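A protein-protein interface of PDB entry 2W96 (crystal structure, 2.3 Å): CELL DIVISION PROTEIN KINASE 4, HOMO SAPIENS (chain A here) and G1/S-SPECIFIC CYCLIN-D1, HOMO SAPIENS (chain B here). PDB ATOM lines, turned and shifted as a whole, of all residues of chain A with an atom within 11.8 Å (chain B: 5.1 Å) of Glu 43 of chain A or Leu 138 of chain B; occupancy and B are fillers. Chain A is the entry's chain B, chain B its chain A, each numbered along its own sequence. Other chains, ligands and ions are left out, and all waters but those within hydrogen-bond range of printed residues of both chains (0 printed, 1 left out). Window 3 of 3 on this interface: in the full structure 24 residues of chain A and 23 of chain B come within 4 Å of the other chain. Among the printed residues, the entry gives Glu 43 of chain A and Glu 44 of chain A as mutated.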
ATOM      1  N   VAL A  39      27.932  19.803  29.869  1.00  0.00           N
ATOM      2  CA  VAL A  39      27.051  20.963  29.840  1.00  0.00           C
ATOM      3  C   VAL A  39      26.066  20.879  30.996  1.00  0.00           C
ATOM      4  O   VAL A  39      25.673  19.788  31.414  1.00  0.00           O
ATOM      5  CB  VAL A  39      26.315  21.083  28.484  1.00  0.00           C
ATOM      6  CG1 VAL A  39      27.308  21.122  27.331  1.00  0.00           C
ATOM      7  CG2 VAL A  39      25.324  19.934  28.315  1.00  0.00           C
ATOM      8  N   PRO A  40      25.627  22.040  31.507  1.00  0.00           N
ATOM      9  CA  PRO A  40      24.694  22.075  32.637  1.00  0.00           C
ATOM     10  C   PRO A  40      23.261  21.783  32.211  1.00  0.00           C
ATOM     11  O   PRO A  40      22.737  22.415  31.295  1.00  0.00           O
ATOM     12  CB  PRO A  40      24.830  23.507  33.161  1.00  0.00           C
ATOM     13  CG  PRO A  40      25.336  24.305  32.019  1.00  0.00           C
ATOM     14  CD  PRO A  40      26.110  23.381  31.128  1.00  0.00           C
ATOM     15  N   ASN A  41      22.640  20.806  32.866  1.00  0.00           N
ATOM     16  CA  ASN A  41      21.256  20.448  32.588  1.00  0.00           C
ATOM     17  C   ASN A  41      20.260  21.325  33.348  1.00  0.00           C
ATOM     18  O   ASN A  41      19.762  20.937  34.403  1.00  0.00           O
ATOM     19  CB  ASN A  41      21.010  18.986  32.939  1.00  0.00           C
ATOM     20  CG  ASN A  41      19.578  18.578  32.724  1.00  0.00           C
ATOM     21  OD1 ASN A  41      18.831  19.260  32.027  1.00  0.00           O
ATOM     22  ND2 ASN A  41      19.177  17.469  33.334  1.00  0.00           N
ATOM     23  N   GLY A  42      19.910  22.468  32.772  1.00  0.00           N
ATOM     24  CA  GLY A  42      19.031  23.422  33.421  1.00  0.00           C
ATOM     25  C   GLY A  42      17.579  23.003  33.582  1.00  0.00           C
ATOM     26  O   GLY A  42      17.219  21.835  33.414  1.00  0.00           O
ATOM     27  N   GLU A  43      16.755  23.985  33.942  1.00  0.00           N
ATOM     28  CA  GLU A  43      15.324  23.808  34.177  1.00  0.00           C
ATOM     29  C   GLU A  43      14.600  23.805  32.832  1.00  0.00           C
ATOM     30  O   GLU A  43      13.458  23.354  32.715  1.00  0.00           O
ATOM     31  CB  GLU A  43      14.814  24.975  35.039  1.00  0.00           C
ATOM     32  CG  GLU A  43      13.308  25.031  35.242  1.00  0.00           C
ATOM     33  CD  GLU A  43      12.869  26.295  35.967  1.00  0.00           C
ATOM     34  OE1 GLU A  43      13.744  26.997  36.521  1.00  0.00           O
ATOM     35  OE2 GLU A  43      11.652  26.588  35.982  1.00  0.00           O
ATOM     36  N   GLU A  44      15.289  24.316  31.819  1.00  0.00           N
ATOM     37  CA  GLU A  44      14.766  24.357  30.467  1.00  0.00           C
ATOM     38  C   GLU A  44      15.492  23.349  29.575  1.00  0.00           C
ATOM     39  O   GLU A  44      15.553  23.513  28.356  1.00  0.00           O
ATOM     40  CB  GLU A  44      14.883  25.772  29.912  1.00  0.00           C
ATOM     41  CG  GLU A  44      13.984  26.767  30.625  1.00  0.00           C
ATOM     42  CD  GLU A  44      12.523  26.347  30.594  1.00  0.00           C
ATOM     43  OE1 GLU A  44      12.057  25.871  29.536  1.00  0.00           O
ATOM     44  OE2 GLU A  44      11.837  26.499  31.628  1.00  0.00           O
ATOM     45  N   GLY A  45      16.013  22.290  30.189  1.00  0.00           N
ATOM     46  CA  GLY A  45      16.675  21.220  29.477  1.00  0.00           C
ATOM     47  C   GLY A  45      18.039  21.641  28.983  1.00  0.00           C
ATOM     48  O   GLY A  45      18.865  22.130  29.748  1.00  0.00           O
ATOM     49  N   LEU A  46      18.250  21.514  27.680  1.00  0.00           N
ATOM     50  CA  LEU A  46      19.548  21.788  27.076  1.00  0.00           C
ATOM     51  C   LEU A  46      19.867  23.269  27.064  1.00  0.00           C
ATOM     52  O   LEU A  46      19.022  24.094  26.726  1.00  0.00           O
ATOM     53  CB  LEU A  46      19.595  21.221  25.661  1.00  0.00           C
ATOM     54  CG  LEU A  46      19.477  19.704  25.649  1.00  0.00           C
ATOM     55  CD1 LEU A  46      19.321  19.200  24.235  1.00  0.00           C
ATOM     56  CD2 LEU A  46      20.696  19.091  26.326  1.00  0.00           C
ATOM     57  N   PRO A  47      21.107  23.623  27.425  1.00  0.00           N
ATOM     58  CA  PRO A  47      21.475  25.043  27.451  1.00  0.00           C
ATOM     59  C   PRO A  47      21.415  25.635  26.049  1.00  0.00           C
ATOM     60  O   PRO A  47      22.088  25.148  25.135  1.00  0.00           O
ATOM     61  CB  PRO A  47      22.921  25.026  27.965  1.00  0.00           C
ATOM     62  CG  PRO A  47      23.080  23.703  28.630  1.00  0.00           C
ATOM     63  CD  PRO A  47      22.216  22.760  27.860  1.00  0.00           C
ATOM     64  N   ILE A  48      20.653  26.717  25.907  1.00  0.00           N
ATOM     65  CA  ILE A  48      20.347  27.283  24.597  1.00  0.00           C
ATOM     66  C   ILE A  48      21.562  27.632  23.759  1.00  0.00           C
ATOM     67  O   ILE A  48      21.545  27.475  22.549  1.00  0.00           O
ATOM     68  CB  ILE A  48      19.394  28.487  24.695  1.00  0.00           C
ATOM     69  CG1 ILE A  48      18.183  28.147  25.557  1.00  0.00           C
ATOM     70  CG2 ILE A  48      18.926  28.901  23.301  1.00  0.00           C
ATOM     71  CD1 ILE A  48      16.979  29.036  25.263  1.00  0.00           C
ATOM     72  N   VAL A  51      22.884  24.535  22.225  1.00  0.00           N
ATOM     73  CA  VAL A  51      22.011  24.149  21.124  1.00  0.00           C
ATOM     74  C   VAL A  51      22.229  25.007  19.890  1.00  0.00           C
ATOM     75  O   VAL A  51      22.391  24.476  18.787  1.00  0.00           O
ATOM     76  CB  VAL A  51      20.522  24.083  21.532  1.00  0.00           C
ATOM     77  CG1 VAL A  51      20.356  23.402  22.869  1.00  0.00           C
ATOM     78  CG2 VAL A  51      19.901  25.460  21.534  1.00  0.00           C
ATOM     79  N   ALA A  76      24.037  13.823  22.892  1.00  0.00           N
ATOM     80  CA  ALA A  76      24.004  14.008  24.335  1.00  0.00           C
ATOM     81  C   ALA A  76      23.902  12.613  24.932  1.00  0.00           C
ATOM     82  O   ALA A  76      22.889  11.942  24.768  1.00  0.00           O
ATOM     83  CB  ALA A  76      22.811  14.859  24.737  1.00  0.00           C
ATOM     84  N   THR A  77      24.991  12.142  25.531  1.00  0.00           N
ATOM     85  CA  THR A  77      25.099  10.743  25.949  1.00  0.00           C
ATOM     86  C   THR A  77      24.631  10.533  27.383  1.00  0.00           C
ATOM     87  O   THR A  77      23.670   9.813  27.631  1.00  0.00           O
ATOM     88  CB  THR A  77      26.535  10.201  25.753  1.00  0.00           C
ATOM     89  OG1 THR A  77      27.408  10.780  26.733  1.00  0.00           O
ATOM     90  CG2 THR A  77      27.054  10.541  24.357  1.00  0.00           C
ATOM     91  N   SER A  78      25.362  11.112  28.326  1.00  0.00           N
ATOM     92  CA  SER A  78      24.989  11.049  29.736  1.00  0.00           C
ATOM     93  C   SER A  78      23.963  12.140  30.042  1.00  0.00           C
ATOM     94  O   SER A  78      23.595  12.911  29.161  1.00  0.00           O
ATOM     95  CB  SER A  78      26.229  11.218  30.620  1.00  0.00           C
ATOM     96  OG  SER A  78      25.867  11.522  31.956  1.00  0.00           O
ATOM     97  N   ARG A  79      23.522  12.206  31.295  1.00  0.00           N
ATOM     98  CA  ARG A  79      22.545  13.200  31.727  1.00  0.00           C
ATOM     99  C   ARG A  79      22.351  13.167  33.239  1.00  0.00           C
ATOM    100  O   ARG A  79      21.855  12.179  33.786  1.00  0.00           O
ATOM    101  CB  ARG A  79      21.194  12.947  31.055  1.00  0.00           C
ATOM    102  CG  ARG A  79      20.996  13.640  29.723  1.00  0.00           C
ATOM    103  CD  ARG A  79      19.636  13.297  29.140  1.00  0.00           C
ATOM    104  NE  ARG A  79      19.457  11.858  28.968  1.00  0.00           N
ATOM    105  CZ  ARG A  79      18.329  11.288  28.555  1.00  0.00           C
ATOM    106  NH1 ARG A  79      17.268  12.035  28.279  1.00  0.00           N
ATOM    107  NH2 ARG A  79      18.258   9.971  28.425  1.00  0.00           N
ATOM    108  N   THR A  80      22.698  14.261  33.908  1.00  0.00           N
ATOM    109  CA  THR A  80      22.382  14.423  35.326  1.00  0.00           C
ATOM    110  C   THR A  80      21.653  15.740  35.578  1.00  0.00           C
ATOM    111  O   THR A  80      21.635  16.623  34.716  1.00  0.00           O
ATOM    112  CB  THR A  80      23.630  14.296  36.214  1.00  0.00           C
ATOM    113  OG1 THR A  80      24.423  15.486  36.101  1.00  0.00           O
ATOM    114  CG2 THR A  80      24.456  13.088  35.800  1.00  0.00           C
ATOM    115  N   ASP A  81      21.065  15.869  36.764  1.00  0.00           N
ATOM    116  CA  ASP A  81      20.275  17.046  37.109  1.00  0.00           C
ATOM    117  C   ASP A  81      21.081  18.335  36.994  1.00  0.00           C
ATOM    118  O   ASP A  81      20.517  19.431  36.947  1.00  0.00           O
ATOM    119  CB  ASP A  81      19.683  16.912  38.514  1.00  0.00           C
ATOM    120  CG  ASP A  81      18.664  15.794  38.612  1.00  0.00           C
ATOM    121  OD1 ASP A  81      18.256  15.265  37.553  1.00  0.00           O
ATOM    122  OD2 ASP A  81      18.263  15.451  39.746  1.00  0.00           O
ATOM    123  N   ARG A  82      22.403  18.197  36.940  1.00  0.00           N
ATOM    124  CA  ARG A  82      23.275  19.349  36.753  1.00  0.00           C
ATOM    125  C   ARG A  82      23.992  19.315  35.411  1.00  0.00           C
ATOM    126  O   ARG A  82      24.429  20.351  34.913  1.00  0.00           O
ATOM    127  CB  ARG A  82      24.312  19.435  37.872  1.00  0.00           C
ATOM    128  CG  ARG A  82      25.236  20.638  37.749  1.00  0.00           C
ATOM    129  CD  ARG A  82      26.137  20.768  38.965  1.00  0.00           C
ATOM    130  NE  ARG A  82      26.350  22.166  39.322  1.00  0.00           N
ATOM    131  CZ  ARG A  82      25.485  22.892  40.025  1.00  0.00           C
ATOM    132  NH1 ARG A  82      25.753  24.160  40.306  1.00  0.00           N
ATOM    133  NH2 ARG A  82      24.349  22.347  40.443  1.00  0.00           N
ATOM    134  N   GLU A  83      24.145  18.125  34.842  1.00  0.00           N
ATOM    135  CA  GLU A  83      24.956  17.985  33.639  1.00  0.00           C
ATOM    136  C   GLU A  83      24.403  17.095  32.533  1.00  0.00           C
ATOM    137  O   GLU A  83      23.673  16.137  32.779  1.00  0.00           O
ATOM    138  CB  GLU A  83      26.393  17.586  33.983  1.00  0.00           C
ATOM    139  CG  GLU A  83      27.209  18.722  34.586  1.00  0.00           C
ATOM    140  CD  GLU A  83      28.655  18.341  34.839  1.00  0.00           C
ATOM    141  OE1 GLU A  83      29.045  17.204  34.497  1.00  0.00           O
ATOM    142  OE2 GLU A  83      29.404  19.188  35.371  1.00  0.00           O
ATOM    143  N   ILE A  84      24.729  17.469  31.302  1.00  0.00           N
ATOM    144  CA  ILE A  84      24.557  16.605  30.144  1.00  0.00           C
ATOM    145  C   ILE A  84      25.907  16.488  29.437  1.00  0.00           C
ATOM    146  O   ILE A  84      26.610  17.480  29.240  1.00  0.00           O
ATOM    147  CB  ILE A  84      23.468  17.147  29.192  1.00  0.00           C
ATOM    148  CG1 ILE A  84      22.158  17.364  29.952  1.00  0.00           C
ATOM    149  CG2 ILE A  84      23.261  16.197  28.025  1.00  0.00           C
ATOM    150  CD1 ILE A  84      21.261  18.398  29.326  1.00  0.00           C
ATOM    151  N   LYS A  85      26.290  15.264  29.103  1.00  0.00           N
ATOM    152  CA  LYS A  85      27.535  15.041  28.394  1.00  0.00           C
ATOM    153  C   LYS A  85      27.241  14.888  26.909  1.00  0.00           C
ATOM    154  O   LYS A  85      26.370  14.113  26.512  1.00  0.00           O
ATOM    155  CB  LYS A  85      28.260  13.819  28.956  1.00  0.00           C
ATOM    156  CG  LYS A  85      29.643  13.570  28.368  1.00  0.00           C
ATOM    157  CD  LYS A  85      29.574  12.659  27.157  1.00  0.00           C
ATOM    158  CE  LYS A  85      30.881  11.907  26.975  1.00  0.00           C
ATOM    159  NZ  LYS A  85      30.761  10.798  25.987  1.00  0.00           N
ATOM    160  N   VAL A  86      27.896  15.720  26.107  1.00  0.00           N
ATOM    161  CA  VAL A  86      27.675  15.733  24.666  1.00  0.00           C
ATOM    162  C   VAL A  86      28.968  15.351  23.964  1.00  0.00           C
ATOM    163  O   VAL A  86      30.003  15.977  24.176  1.00  0.00           O
ATOM    164  CB  VAL A  86      27.188  17.127  24.185  1.00  0.00           C
ATOM    165  CG1 VAL A  86      27.158  17.188  22.660  1.00  0.00           C
ATOM    166  CG2 VAL A  86      25.826  17.459  24.775  1.00  0.00           C
ATOM    167  N   PHE B 108       9.411  23.611  21.431  1.00  0.00           N
ATOM    168  CA  PHE B 108      10.365  23.957  22.479  1.00  0.00           C
ATOM    169  C   PHE B 108      11.774  24.159  21.906  1.00  0.00           C
ATOM    170  O   PHE B 108      12.398  25.197  22.119  1.00  0.00           O
ATOM    171  CB  PHE B 108      10.365  22.835  23.519  1.00  0.00           C
ATOM    172  CG  PHE B 108      11.179  23.127  24.743  1.00  0.00           C
ATOM    173  CD1 PHE B 108      10.812  24.151  25.616  1.00  0.00           C
ATOM    174  CD2 PHE B 108      12.280  22.341  25.058  1.00  0.00           C
ATOM    175  CE1 PHE B 108      11.549  24.394  26.772  1.00  0.00           C
ATOM    176  CE2 PHE B 108      13.007  22.573  26.213  1.00  0.00           C
ATOM    177  CZ  PHE B 108      12.648  23.610  27.066  1.00  0.00           C
ATOM    178  N   ALA B 121       9.352  25.180  29.174  1.00  0.00           N
ATOM    179  CA  ALA B 121       8.769  23.841  29.226  1.00  0.00           C
ATOM    180  C   ALA B 121       7.390  23.861  29.899  1.00  0.00           C
ATOM    181  O   ALA B 121       6.466  23.151  29.495  1.00  0.00           O
ATOM    182  CB  ALA B 121       9.706  22.888  29.960  1.00  0.00           C
ATOM    183  N   PRO B 134       6.759  18.830  32.373  1.00  0.00           N
ATOM    184  CA  PRO B 134       8.065  19.333  31.931  1.00  0.00           C
ATOM    185  C   PRO B 134       9.139  18.255  31.788  1.00  0.00           C
ATOM    186  O   PRO B 134       9.887  18.253  30.810  1.00  0.00           O
ATOM    187  CB  PRO B 134       8.439  20.336  33.024  1.00  0.00           C
ATOM    188  CG  PRO B 134       7.128  20.856  33.490  1.00  0.00           C
ATOM    189  CD  PRO B 134       6.161  19.697  33.403  1.00  0.00           C
ATOM    190  N   GLU B 135       9.220  17.341  32.750  1.00  0.00           N
ATOM    191  CA  GLU B 135      10.261  16.317  32.707  1.00  0.00           C
ATOM    192  C   GLU B 135      10.069  15.422  31.487  1.00  0.00           C
ATOM    193  O   GLU B 135      11.034  14.916  30.916  1.00  0.00           O
ATOM    194  CB  GLU B 135      10.271  15.483  33.983  1.00  0.00           C
ATOM    195  CG  GLU B 135       9.888  16.266  35.226  1.00  0.00           C
ATOM    196  CD  GLU B 135       8.399  16.200  35.519  1.00  0.00           C
ATOM    197  OE1 GLU B 135       7.841  15.081  35.501  1.00  0.00           O
ATOM    198  OE2 GLU B 135       7.800  17.259  35.807  1.00  0.00           O
ATOM    199  N   GLU B 136       8.815  15.234  31.087  1.00  0.00           N
ATOM    200  CA  GLU B 136       8.522  14.496  29.870  1.00  0.00           C
ATOM    201  C   GLU B 136       9.068  15.250  28.661  1.00  0.00           C
ATOM    202  O   GLU B 136       9.667  14.664  27.761  1.00  0.00           O
ATOM    203  CB  GLU B 136       7.015  14.312  29.718  1.00  0.00           C
ATOM    204  CG  GLU B 136       6.422  13.239  30.611  1.00  0.00           C
ATOM    205  CD  GLU B 136       4.944  13.070  30.379  1.00  0.00           C
ATOM    206  OE1 GLU B 136       4.210  14.072  30.500  1.00  0.00           O
ATOM    207  OE2 GLU B 136       4.522  11.945  30.044  1.00  0.00           O
ATOM    208  N   LEU B 137       8.828  16.555  28.648  1.00  0.00           N
ATOM    209  CA  LEU B 137       9.302  17.426  27.584  1.00  0.00           C
ATOM    210  C   LEU B 137      10.835  17.417  27.537  1.00  0.00           C
ATOM    211  O   LEU B 137      11.432  17.284  26.472  1.00  0.00           O
ATOM    212  CB  LEU B 137       8.792  18.847  27.828  1.00  0.00           C
ATOM    213  CG  LEU B 137       8.827  19.847  26.673  1.00  0.00           C
ATOM    214  CD1 LEU B 137       7.517  19.804  25.908  1.00  0.00           C
ATOM    215  CD2 LEU B 137       9.069  21.228  27.227  1.00  0.00           C
ATOM    216  N   LEU B 138      11.465  17.536  28.700  1.00  0.00           N
ATOM    217  CA  LEU B 138      12.920  17.597  28.771  1.00  0.00           C
ATOM    218  C   LEU B 138      13.567  16.311  28.283  1.00  0.00           C
ATOM    219  O   LEU B 138      14.655  16.332  27.703  1.00  0.00           O
ATOM    220  CB  LEU B 138      13.387  17.918  30.191  1.00  0.00           C
ATOM    221  CG  LEU B 138      12.898  19.245  30.773  1.00  0.00           C
ATOM    222  CD1 LEU B 138      13.728  19.623  31.994  1.00  0.00           C
ATOM    223  CD2 LEU B 138      12.929  20.352  29.706  1.00  0.00           C
ATOM    224  N   GLN B 139      12.904  15.192  28.538  1.00  0.00           N
ATOM    225  CA  GLN B 139      13.385  13.902  28.069  1.00  0.00           C
ATOM    226  C   GLN B 139      13.199  13.711  26.566  1.00  0.00           C
ATOM    227  O   GLN B 139      14.098  13.203  25.892  1.00  0.00           O
ATOM    228  CB  GLN B 139      12.737  12.758  28.854  1.00  0.00           C
ATOM    229  CG  GLN B 139      13.254  12.626  30.286  1.00  0.00           C
ATOM    230  CD  GLN B 139      12.497  11.577  31.091  1.00  0.00           C
ATOM    231  OE1 GLN B 139      12.501  11.600  32.322  1.00  0.00           O
ATOM    232  NE2 GLN B 139      11.842  10.654  30.394  1.00  0.00           N
ATOM    233  N   MET B 140      12.041  14.115  26.041  1.00  0.00           N
ATOM    234  CA  MET B 140      11.831  14.135  24.586  1.00  0.00           C
ATOM    235  C   MET B 140      12.842  15.023  23.866  1.00  0.00           C
ATOM    236  O   MET B 140      13.348  14.657  22.804  1.00  0.00           O
ATOM    237  CB  MET B 140      10.410  14.563  24.222  1.00  0.00           C
ATOM    238  CG  MET B 140       9.456  13.429  23.935  1.00  0.00           C
ATOM    239  SD  MET B 140       9.892  12.458  22.477  1.00  0.00           S
ATOM    240  CE  MET B 140       8.232  11.783  22.026  1.00  0.00           C
ATOM    241  N   GLU B 141      13.149  16.180  24.441  1.00  0.00           N
ATOM    242  CA  GLU B 141      14.067  17.111  23.776  1.00  0.00           C
ATOM    243  C   GLU B 141      15.394  16.452  23.416  1.00  0.00           C
ATOM    244  O   GLU B 141      15.942  16.682  22.341  1.00  0.00           O
ATOM    245  CB  GLU B 141      14.321  18.387  24.598  1.00  0.00           C
ATOM    246  CG  GLU B 141      15.345  19.286  23.923  1.00  0.00           C
ATOM    247  CD  GLU B 141      15.844  20.437  24.772  1.00  0.00           C
ATOM    248  OE1 GLU B 141      16.120  20.238  25.971  1.00  0.00           O
ATOM    249  OE2 GLU B 141      16.089  21.518  24.195  1.00  0.00           O
ATOM    250  N   LEU B 142      15.933  15.671  24.340  1.00  0.00           N
ATOM    251  CA  LEU B 142      17.184  14.975  24.100  1.00  0.00           C
ATOM    252  C   LEU B 142      17.058  13.907  23.014  1.00  0.00           C
ATOM    253  O   LEU B 142      17.920  13.794  22.133  1.00  0.00           O
ATOM    254  CB  LEU B 142      17.696  14.386  25.406  1.00  0.00           C
ATOM    255  CG  LEU B 142      18.135  15.501  26.355  1.00  0.00           C
ATOM    256  CD1 LEU B 142      17.766  15.184  27.803  1.00  0.00           C
ATOM    257  CD2 LEU B 142      19.628  15.759  26.212  1.00  0.00           C
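The backbone NH of Ala 121 of chain B sits at hydrogen-bond distance from the side-chain carboxylate of Glu 44 of chain A (2.8 Å).
OE1 of Glu 141 of chain B lies within hydrogen-bond range of N of Leu 46 of chain A (3.0 Å).
Of the printed residues of chain B, Glu 43 of chain A touches Leu 138.
Printed residues of chain A within 4 Å of Leu 138 of chain B: Glu 43 (3.8 Å), Glu 44 (3.9 Å) and Gly 45 (3.7 Å).
No residue of chain A comes within 4 Å of Pro 134 of chain B.
No residue of chain A comes within 4 Å of Leu 137 of chain B.
Gln 139 of chain B touches none of the printed residues of chain A.
Printed residues of chain A within 4 Å of Glu 141 of chain B: Gly 45 and Leu 46.
Leu 142 of chain B touches just these residues of chain A: Leu 46, Ala 76 and Arg 79.
Of the printed residues of chain B, Glu 44 of chain A touches Phe 108, Ala 121 and Leu 138.
Printed residues of chain B within 4 Å of Leu 46 of chain A: Glu 141 (3.0 Å) and Leu 142 (3.5 Å).
Printed residues of chain B within 4 Å of Arg 79 of chain A: Leu 142.
Printed residues of chain A within 4 Å of Phe 108 of chain B: Glu 44 (3.2 Å).
Printed residues of chain B within 4 Å of Gly 45 of chain A: Leu 138 (3.7 Å) and Glu 141 (3.7 Å).
Ser 78 of chain A touches none of the printed residues of chain B.
The nearest residue of chain B that does not touch Glu 43 of chain A is Ala 121 of chain B (4.7 Å).
The nearest printed residue of chain B that does not touch Ala 76 of chain A is Glu 141 of chain B (7.5 Å).
Of the 11 printed residues of chain B, 5 touch a printed residue of chain A.
Among the printed residues, 10 pairs touch across the chains.
Among the printed residues, no Asp or Glu carboxylate lies within 4 Å of a Lys or Arg side-chain nitrogen of the other chain.
Among the printed residues, pairs that only touch across the chains: Arg 79 of chain A with Leu 142 of chain B (3.0 Å), Glu 44 of chain A with Phe 108 of chain B (3.2 Å), Leu 46 of chain A with Leu 142 of chain B (3.5 Å), Ala 76 of chain A with Leu 142 of chain B (3.6 Å), Gly 45 of chain A with Leu 138 of chain B (3.7 Å), Gly 45 of chain A with Glu 141 of chain B (3.7 Å), Glu 43 of chain A with Leu 138 of chain B (3.8 Å) and Glu 44 of chain A with Leu 138 of chain B (3.9 Å).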
